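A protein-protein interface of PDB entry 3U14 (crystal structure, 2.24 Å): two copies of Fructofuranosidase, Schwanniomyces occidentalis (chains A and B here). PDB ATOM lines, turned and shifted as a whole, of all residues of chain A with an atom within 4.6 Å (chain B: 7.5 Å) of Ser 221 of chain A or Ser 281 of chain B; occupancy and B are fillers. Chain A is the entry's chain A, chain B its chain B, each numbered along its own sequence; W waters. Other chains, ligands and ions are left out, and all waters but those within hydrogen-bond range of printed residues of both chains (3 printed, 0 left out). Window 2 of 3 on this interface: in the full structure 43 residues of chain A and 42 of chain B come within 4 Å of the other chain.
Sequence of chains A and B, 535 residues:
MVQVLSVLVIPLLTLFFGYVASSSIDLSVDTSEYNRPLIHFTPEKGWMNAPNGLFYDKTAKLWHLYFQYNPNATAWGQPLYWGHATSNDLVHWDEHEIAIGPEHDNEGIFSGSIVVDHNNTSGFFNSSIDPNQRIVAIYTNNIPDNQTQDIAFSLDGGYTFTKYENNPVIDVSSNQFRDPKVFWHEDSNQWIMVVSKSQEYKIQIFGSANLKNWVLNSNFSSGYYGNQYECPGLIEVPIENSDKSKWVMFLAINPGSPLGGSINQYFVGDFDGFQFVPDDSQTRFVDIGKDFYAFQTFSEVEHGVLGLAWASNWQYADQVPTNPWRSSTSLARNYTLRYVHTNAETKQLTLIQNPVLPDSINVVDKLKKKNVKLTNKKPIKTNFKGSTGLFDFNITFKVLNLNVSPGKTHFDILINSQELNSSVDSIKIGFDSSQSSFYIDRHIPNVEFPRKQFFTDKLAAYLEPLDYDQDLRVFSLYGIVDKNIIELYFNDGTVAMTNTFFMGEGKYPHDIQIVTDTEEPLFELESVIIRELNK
The side-chain hydroxyl (OG) of Ser 222 of chain A is in hydrogen-bond range of the side-chain hydroxyl (OG) of Ser 281 of chain B (2.7 Å). O of Gly 223 of chain A sits at hydrogen-bond distance from N of Thr 283 of chain B (2.9 Å). The side-chain hydroxyl (OG) of Ser 281 of chain A is in hydrogen-bond range of the side-chain hydroxyl (OG) of Ser 222 of chain B, at 2.8 Å.
The side-chain hydroxyl (OG) of Ser 221 of chain A is in hydrogen-bond range of the backbone carbonyl oxygen (O) of Tyr 201 of chain A, 2.6 Å away. The backbone carbonyl oxygen of Ser 222 of chain A sits at hydrogen-bond distance from the side-chain hydroxyl of Tyr 229 of chain A, 2.6 Å away. The side-chain amide nitrogen (NE2) of Gln 282 of chain B lies within hydrogen-bond range of the side-chain carboxylate (OD1) of Asp 280 of chain B (2.8 Å).
OG of Ser 281 of chain B touches O of Ser 221 of chain A, 3.6 Å away. N of Gly 223 of chain A touches O of Ser 281 of chain B, 3.6 Å away. Gln 282 of chain B touches Gly 223 of chain A. Gln 282 of chain B touches Tyr 225 of chain A (OE1 to CD2, 3.6 Å). Ser 281 of chain A touches Gly 223 of chain B (O to N, 3.6 Å).
Ser 221 of chain A touches just one residue of chain B: Ser 281. Of the printed residues of chain B, Tyr 225 of chain A touches Gln 282 (3.6 Å). Of the printed residues of chain B, Gly 223 of chain A touches Ser 281, Gln 282 and Thr 283. Of the printed residues of chain A, Ser 222 of chain B touches Ser 281 (2.8 Å). Of the printed residues of chain A, Gly 223 of chain B touches Ser 281. Asn 219 of chain A touches none of the printed residues of chain B. The nearest printed residue of chain B that does not touch Gly 223 of chain A is Arg 284 of chain B (5.9 Å).
Ser 222 of chain A touches Ser 281 of chain B, and with the chains exchanged Ser 281 of chain A touches Ser 222 of chain B. Gly 223 of chain A touches Ser 281 of chain B, and with the chains exchanged Ser 281 of chain A touches Gly 223 of chain B. 3 positions are printed for both chains.
Water W2 lies within hydrogen-bond range of the backbone carbonyl oxygen of Ser 281 of chain B (2.5 Å), the backbone carbonyl oxygen of Ser 281 of chain A (2.8 Å) and the side-chain hydroxyl of Thr 283 of chain B (2.9 Å). Water W3 lies within hydrogen-bond range of OH of Tyr 225 of chain A (2.6 Å), O of Ser 221 of chain A (3.0 Å) and N of Ser 281 of chain B (3.1 Å). Water W1 lies within hydrogen-bond range of the backbone carbonyl oxygen of Thr 283 of chain B, the side-chain amide oxygen of Gln 282 of chain B and the backbone NH of Tyr 225 of chain A.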
ATOM      1  N   TYR A 201      12.968  -4.155  10.409  1.00  0.00           N
ATOM      2  CA  TYR A 201      13.234  -3.087   9.443  1.00  0.00           C
ATOM      3  C   TYR A 201      14.136  -2.017  10.052  1.00  0.00           C
ATOM      4  O   TYR A 201      13.851  -0.822   9.951  1.00  0.00           O
ATOM      5  CB  TYR A 201      11.944  -2.440   8.933  1.00  0.00           C
ATOM      6  CG  TYR A 201      10.953  -3.362   8.280  1.00  0.00           C
ATOM      7  CD1 TYR A 201       9.758  -3.665   8.910  1.00  0.00           C
ATOM      8  CD2 TYR A 201      11.180  -3.891   6.989  1.00  0.00           C
ATOM      9  CE1 TYR A 201       8.801  -4.502   8.291  1.00  0.00           C
ATOM     10  CE2 TYR A 201      10.232  -4.728   6.373  1.00  0.00           C
ATOM     11  CZ  TYR A 201       9.051  -5.024   7.036  1.00  0.00           C
ATOM     12  OH  TYR A 201       8.110  -5.841   6.464  1.00  0.00           O
ATOM     13  N   LYS A 202      15.237  -2.452  10.659  1.00  0.00           N
ATOM     14  CA  LYS A 202      16.237  -1.542  11.197  1.00  0.00           C
ATOM     15  C   LYS A 202      17.596  -1.907  10.677  1.00  0.00           C
ATOM     16  O   LYS A 202      17.988  -3.092  10.683  1.00  0.00           O
ATOM     17  CB  LYS A 202      16.282  -1.610  12.733  1.00  0.00           C
ATOM     18  CG  LYS A 202      14.971  -1.268  13.405  1.00  0.00           C
ATOM     19  CD  LYS A 202      15.106  -1.264  14.911  1.00  0.00           C
ATOM     20  CE  LYS A 202      13.731  -1.094  15.543  1.00  0.00           C
ATOM     21  NZ  LYS A 202      13.831  -0.829  17.003  1.00  0.00           N
ATOM     22  N   ASN A 219      19.871   2.920  15.410  1.00  0.00           N
ATOM     23  CA  ASN A 219      18.999   2.198  14.488  1.00  0.00           C
ATOM     24  C   ASN A 219      18.564   3.120  13.356  1.00  0.00           C
ATOM     25  O   ASN A 219      18.212   4.276  13.591  1.00  0.00           O
ATOM     26  CB  ASN A 219      17.738   1.735  15.215  1.00  0.00           C
ATOM     27  CG  ASN A 219      18.019   0.719  16.310  1.00  0.00           C
ATOM     28  OD1 ASN A 219      18.913  -0.130  16.184  1.00  0.00           O
ATOM     29  ND2 ASN A 219      17.252   0.785  17.380  1.00  0.00           N
ATOM     30  N   PHE A 220      18.569   2.615  12.126  1.00  0.00           N
ATOM     31  CA  PHE A 220      18.066   3.403  11.002  1.00  0.00           C
ATOM     32  C   PHE A 220      16.971   2.664  10.235  1.00  0.00           C
ATOM     33  O   PHE A 220      17.134   1.480   9.880  1.00  0.00           O
ATOM     34  CB  PHE A 220      19.200   3.821  10.073  1.00  0.00           C
ATOM     35  CG  PHE A 220      18.757   4.630   8.888  1.00  0.00           C
ATOM     36  CD1 PHE A 220      18.425   5.968   9.025  1.00  0.00           C
ATOM     37  CD2 PHE A 220      18.711   4.056   7.613  1.00  0.00           C
ATOM     38  CE1 PHE A 220      18.024   6.726   7.918  1.00  0.00           C
ATOM     39  CE2 PHE A 220      18.312   4.804   6.492  1.00  0.00           C
ATOM     40  CZ  PHE A 220      17.971   6.141   6.650  1.00  0.00           C
ATOM     41  N   SER A 221      15.879   3.389   9.976  1.00  0.00           N
ATOM     42  CA  SER A 221      14.707   2.862   9.306  1.00  0.00           C
ATOM     43  C   SER A 221      14.153   3.836   8.288  1.00  0.00           C
ATOM     44  O   SER A 221      13.756   4.938   8.649  1.00  0.00           O
ATOM     45  CB  SER A 221      13.612   2.589  10.327  1.00  0.00           C
ATOM     46  OG  SER A 221      13.953   1.473  11.096  1.00  0.00           O
ATOM     47  N   SER A 222      14.064   3.409   7.035  1.00  0.00           N
ATOM     48  CA  SER A 222      13.555   4.275   5.988  1.00  0.00           C
ATOM     49  C   SER A 222      13.347   3.510   4.678  1.00  0.00           C
ATOM     50  O   SER A 222      13.558   2.281   4.610  1.00  0.00           O
ATOM     51  CB  SER A 222      14.516   5.445   5.747  1.00  0.00           C
ATOM     52  OG  SER A 222      13.862   6.441   4.989  1.00  0.00           O
ATOM     53  N   GLY A 223      12.935   4.238   3.649  1.00  0.00           N
ATOM     54  CA  GLY A 223      12.916   3.709   2.294  1.00  0.00           C
ATOM     55  C   GLY A 223      11.788   2.742   2.016  1.00  0.00           C
ATOM     56  O   GLY A 223      10.697   2.882   2.552  1.00  0.00           O
ATOM     57  N   TYR A 225      10.401  -0.692   2.561  1.00  0.00           N
ATOM     58  CA  TYR A 225      10.513  -1.809   3.511  1.00  0.00           C
ATOM     59  C   TYR A 225      10.135  -2.946   2.632  1.00  0.00           C
ATOM     60  O   TYR A 225       9.386  -2.778   1.776  1.00  0.00           O
ATOM     61  CB  TYR A 225       9.424  -1.679   4.582  1.00  0.00           C
ATOM     62  CG  TYR A 225       9.669  -0.635   5.675  1.00  0.00           C
ATOM     63  CD1 TYR A 225      10.616   0.388   5.524  1.00  0.00           C
ATOM     64  CD2 TYR A 225       8.923  -0.666   6.857  1.00  0.00           C
ATOM     65  CE1 TYR A 225      10.824   1.333   6.542  1.00  0.00           C
ATOM     66  CE2 TYR A 225       9.129   0.265   7.878  1.00  0.00           C
ATOM     67  CZ  TYR A 225      10.068   1.265   7.710  1.00  0.00           C
ATOM     68  OH  TYR A 225      10.240   2.183   8.732  1.00  0.00           O
ATOM     69  N   TYR A 229      14.697  -6.282   5.787  1.00  0.00           N
ATOM     70  CA  TYR A 229      15.974  -5.590   5.535  1.00  0.00           C
ATOM     71  C   TYR A 229      17.125  -6.599   5.492  1.00  0.00           C
ATOM     72  O   TYR A 229      17.197  -7.500   6.325  1.00  0.00           O
ATOM     73  CB  TYR A 229      16.293  -4.597   6.665  1.00  0.00           C
ATOM     74  CG  TYR A 229      15.691  -3.194   6.604  1.00  0.00           C
ATOM     75  CD1 TYR A 229      14.556  -2.907   5.841  1.00  0.00           C
ATOM     76  CD2 TYR A 229      16.254  -2.159   7.369  1.00  0.00           C
ATOM     77  CE1 TYR A 229      14.022  -1.621   5.809  1.00  0.00           C
ATOM     78  CE2 TYR A 229      15.727  -0.889   7.354  1.00  0.00           C
ATOM     79  CZ  TYR A 229      14.620  -0.624   6.585  1.00  0.00           C
ATOM     80  OH  TYR A 229      14.117   0.657   6.595  1.00  0.00           O
ATOM     81  N   SER A 281      14.315  12.327   2.588  1.00  0.00           N
ATOM     82  CA  SER A 281      13.686  11.058   2.934  1.00  0.00           C
ATOM     83  C   SER A 281      13.157  10.295   1.708  1.00  0.00           C
ATOM     84  O   SER A 281      12.207   9.503   1.822  1.00  0.00           O
ATOM     85  CB  SER A 281      12.609  11.277   3.996  1.00  0.00           C
ATOM     86  OG  SER A 281      11.544  12.064   3.505  1.00  0.00           O
ATOM     87  N   SER B 222       8.759  13.806   0.311  1.00  0.00           N
ATOM     88  CA  SER B 222       9.164  12.468   0.723  1.00  0.00           C
ATOM     89  C   SER B 222       8.864  11.408  -0.339  1.00  0.00           C
ATOM     90  O   SER B 222       8.362  11.707  -1.420  1.00  0.00           O
ATOM     91  CB  SER B 222       8.451  12.100   2.027  1.00  0.00           C
ATOM     92  OG  SER B 222       9.103  11.043   2.703  1.00  0.00           O
ATOM     93  N   GLY B 223       9.191  10.167  -0.011  1.00  0.00           N
ATOM     94  CA  GLY B 223       8.770   9.014  -0.804  1.00  0.00           C
ATOM     95  C   GLY B 223       9.538   8.813  -2.085  1.00  0.00           C
ATOM     96  O   GLY B 223      10.747   9.052  -2.152  1.00  0.00           O
ATOM     97  N   PHE B 267       1.333   8.323   2.350  1.00  0.00           N
ATOM     98  CA  PHE B 267       2.030   8.439   3.616  1.00  0.00           C
ATOM     99  C   PHE B 267       1.004   8.511   4.743  1.00  0.00           C
ATOM    100  O   PHE B 267      -0.041   9.120   4.580  1.00  0.00           O
ATOM    101  CB  PHE B 267       2.884   9.721   3.646  1.00  0.00           C
ATOM    102  CG  PHE B 267       3.706   9.947   2.410  1.00  0.00           C
ATOM    103  CD1 PHE B 267       5.007   9.468   2.326  1.00  0.00           C
ATOM    104  CD2 PHE B 267       3.192  10.684   1.339  1.00  0.00           C
ATOM    105  CE1 PHE B 267       5.788   9.711   1.187  1.00  0.00           C
ATOM    106  CE2 PHE B 267       3.960  10.924   0.194  1.00  0.00           C
ATOM    107  CZ  PHE B 267       5.263  10.433   0.118  1.00  0.00           C
ATOM    108  N   VAL B 268       1.318   7.910   5.888  1.00  0.00           N
ATOM    109  CA  VAL B 268       0.416   7.888   7.046  1.00  0.00           C
ATOM    110  C   VAL B 268       1.023   8.720   8.185  1.00  0.00           C
ATOM    111  O   VAL B 268       2.211   8.565   8.514  1.00  0.00           O
ATOM    112  CB  VAL B 268       0.146   6.442   7.514  1.00  0.00           C
ATOM    113  CG1 VAL B 268      -0.778   6.405   8.716  1.00  0.00           C
ATOM    114  CG2 VAL B 268      -0.451   5.634   6.383  1.00  0.00           C
ATOM    115  N   PRO B 278       4.527  12.656   8.896  1.00  0.00           N
ATOM    116  CA  PRO B 278       4.351  11.211   8.729  1.00  0.00           C
ATOM    117  C   PRO B 278       4.877  10.430   9.936  1.00  0.00           C
ATOM    118  O   PRO B 278       5.824  10.870  10.590  1.00  0.00           O
ATOM    119  CB  PRO B 278       5.176  10.905   7.488  1.00  0.00           C
ATOM    120  CG  PRO B 278       6.261  11.948   7.501  1.00  0.00           C
ATOM    121  CD  PRO B 278       5.627  13.193   8.070  1.00  0.00           C
ATOM    122  N   ASP B 279       4.258   9.292  10.230  1.00  0.00           N
ATOM    123  CA  ASP B 279       4.652   8.458  11.359  1.00  0.00           C
ATOM    124  C   ASP B 279       6.008   7.757  11.164  1.00  0.00           C
ATOM    125  O   ASP B 279       6.679   7.418  12.132  1.00  0.00           O
ATOM    126  CB  ASP B 279       3.576   7.421  11.650  1.00  0.00           C
ATOM    127  CG  ASP B 279       2.391   8.000  12.393  1.00  0.00           C
ATOM    128  OD1 ASP B 279       2.434   9.184  12.842  1.00  0.00           O
ATOM    129  OD2 ASP B 279       1.398   7.260  12.524  1.00  0.00           O
ATOM    130  N   ASP B 280       6.388   7.546   9.908  1.00  0.00           N
ATOM    131  CA  ASP B 280       7.684   6.985   9.558  1.00  0.00           C
ATOM    132  C   ASP B 280       8.114   7.653   8.269  1.00  0.00           C
ATOM    133  O   ASP B 280       7.467   8.607   7.842  1.00  0.00           O
ATOM    134  CB  ASP B 280       7.590   5.455   9.406  1.00  0.00           C
ATOM    135  CG  ASP B 280       6.495   5.012   8.428  1.00  0.00           C
ATOM    136  OD1 ASP B 280       5.927   3.933   8.659  1.00  0.00           O
ATOM    137  OD2 ASP B 280       6.199   5.716   7.432  1.00  0.00           O
ATOM    138  N   SER B 281       9.192   7.176   7.652  1.00  0.00           N
ATOM    139  CA  SER B 281       9.632   7.708   6.353  1.00  0.00           C
ATOM    140  C   SER B 281       9.634   6.635   5.231  1.00  0.00           C
ATOM    141  O   SER B 281      10.375   6.711   4.253  1.00  0.00           O
ATOM    142  CB  SER B 281      10.984   8.425   6.494  1.00  0.00           C
ATOM    143  OG  SER B 281      12.043   7.510   6.718  1.00  0.00           O
ATOM    144  N   GLN B 282       8.756   5.647   5.349  1.00  0.00           N
ATOM    145  CA  GLN B 282       8.708   4.611   4.333  1.00  0.00           C
ATOM    146  C   GLN B 282       7.890   5.010   3.116  1.00  0.00           C
ATOM    147  O   GLN B 282       6.978   5.824   3.206  1.00  0.00           O
ATOM    148  CB  GLN B 282       8.210   3.292   4.915  1.00  0.00           C
ATOM    149  CG  GLN B 282       6.696   3.214   5.129  1.00  0.00           C
ATOM    150  CD  GLN B 282       6.274   1.843   5.622  1.00  0.00           C
ATOM    151  OE1 GLN B 282       6.365   0.846   4.896  1.00  0.00           O
ATOM    152  NE2 GLN B 282       5.845   1.777   6.865  1.00  0.00           N
ATOM    153  N   THR B 283       8.246   4.419   1.977  1.00  0.00           N
ATOM    154  CA  THR B 283       7.540   4.621   0.730  1.00  0.00           C
ATOM    155  C   THR B 283       6.598   3.442   0.532  1.00  0.00           C
ATOM    156  O   THR B 283       6.991   2.282   0.732  1.00  0.00           O
ATOM    157  CB  THR B 283       8.537   4.717  -0.445  1.00  0.00           C
ATOM    158  OG1 THR B 283       9.176   5.998  -0.421  1.00  0.00           O
ATOM    159  CG2 THR B 283       7.844   4.554  -1.775  1.00  0.00           C
ATOM    160  N   ARG B 284       5.352   3.753   0.186  1.00  0.00           N
ATOM    161  CA  ARG B 284       4.322   2.748  -0.152  1.00  0.00           C
ATOM    162  C   ARG B 284       3.410   3.233  -1.274  1.00  0.00           C
ATOM    163  O   ARG B 284       3.034   4.412  -1.330  1.00  0.00           O
ATOM    164  CB  ARG B 284       3.474   2.367   1.071  1.00  0.00           C
ATOM    165  CG  ARG B 284       4.211   1.564   2.111  1.00  0.00           C
ATOM    166  CD  ARG B 284       3.399   1.333   3.360  1.00  0.00           C
ATOM    167  NE  ARG B 284       3.262   2.518   4.212  1.00  0.00           N
ATOM    168  CZ  ARG B 284       2.693   2.519   5.429  1.00  0.00           C
ATOM    169  NH1 ARG B 284       2.195   1.405   5.954  1.00  0.00           N
ATOM    170  NH2 ARG B 284       2.599   3.647   6.121  1.00  0.00           N
HETATM  171  O   HOH W   1       7.672   0.433   2.560  1.00  0.00           O
HETATM  172  O   HOH W   2      10.717   7.160   1.795  1.00  0.00           O
HETATM  173  O   HOH W   3      10.812   4.715   8.606  1.00  0.00           O
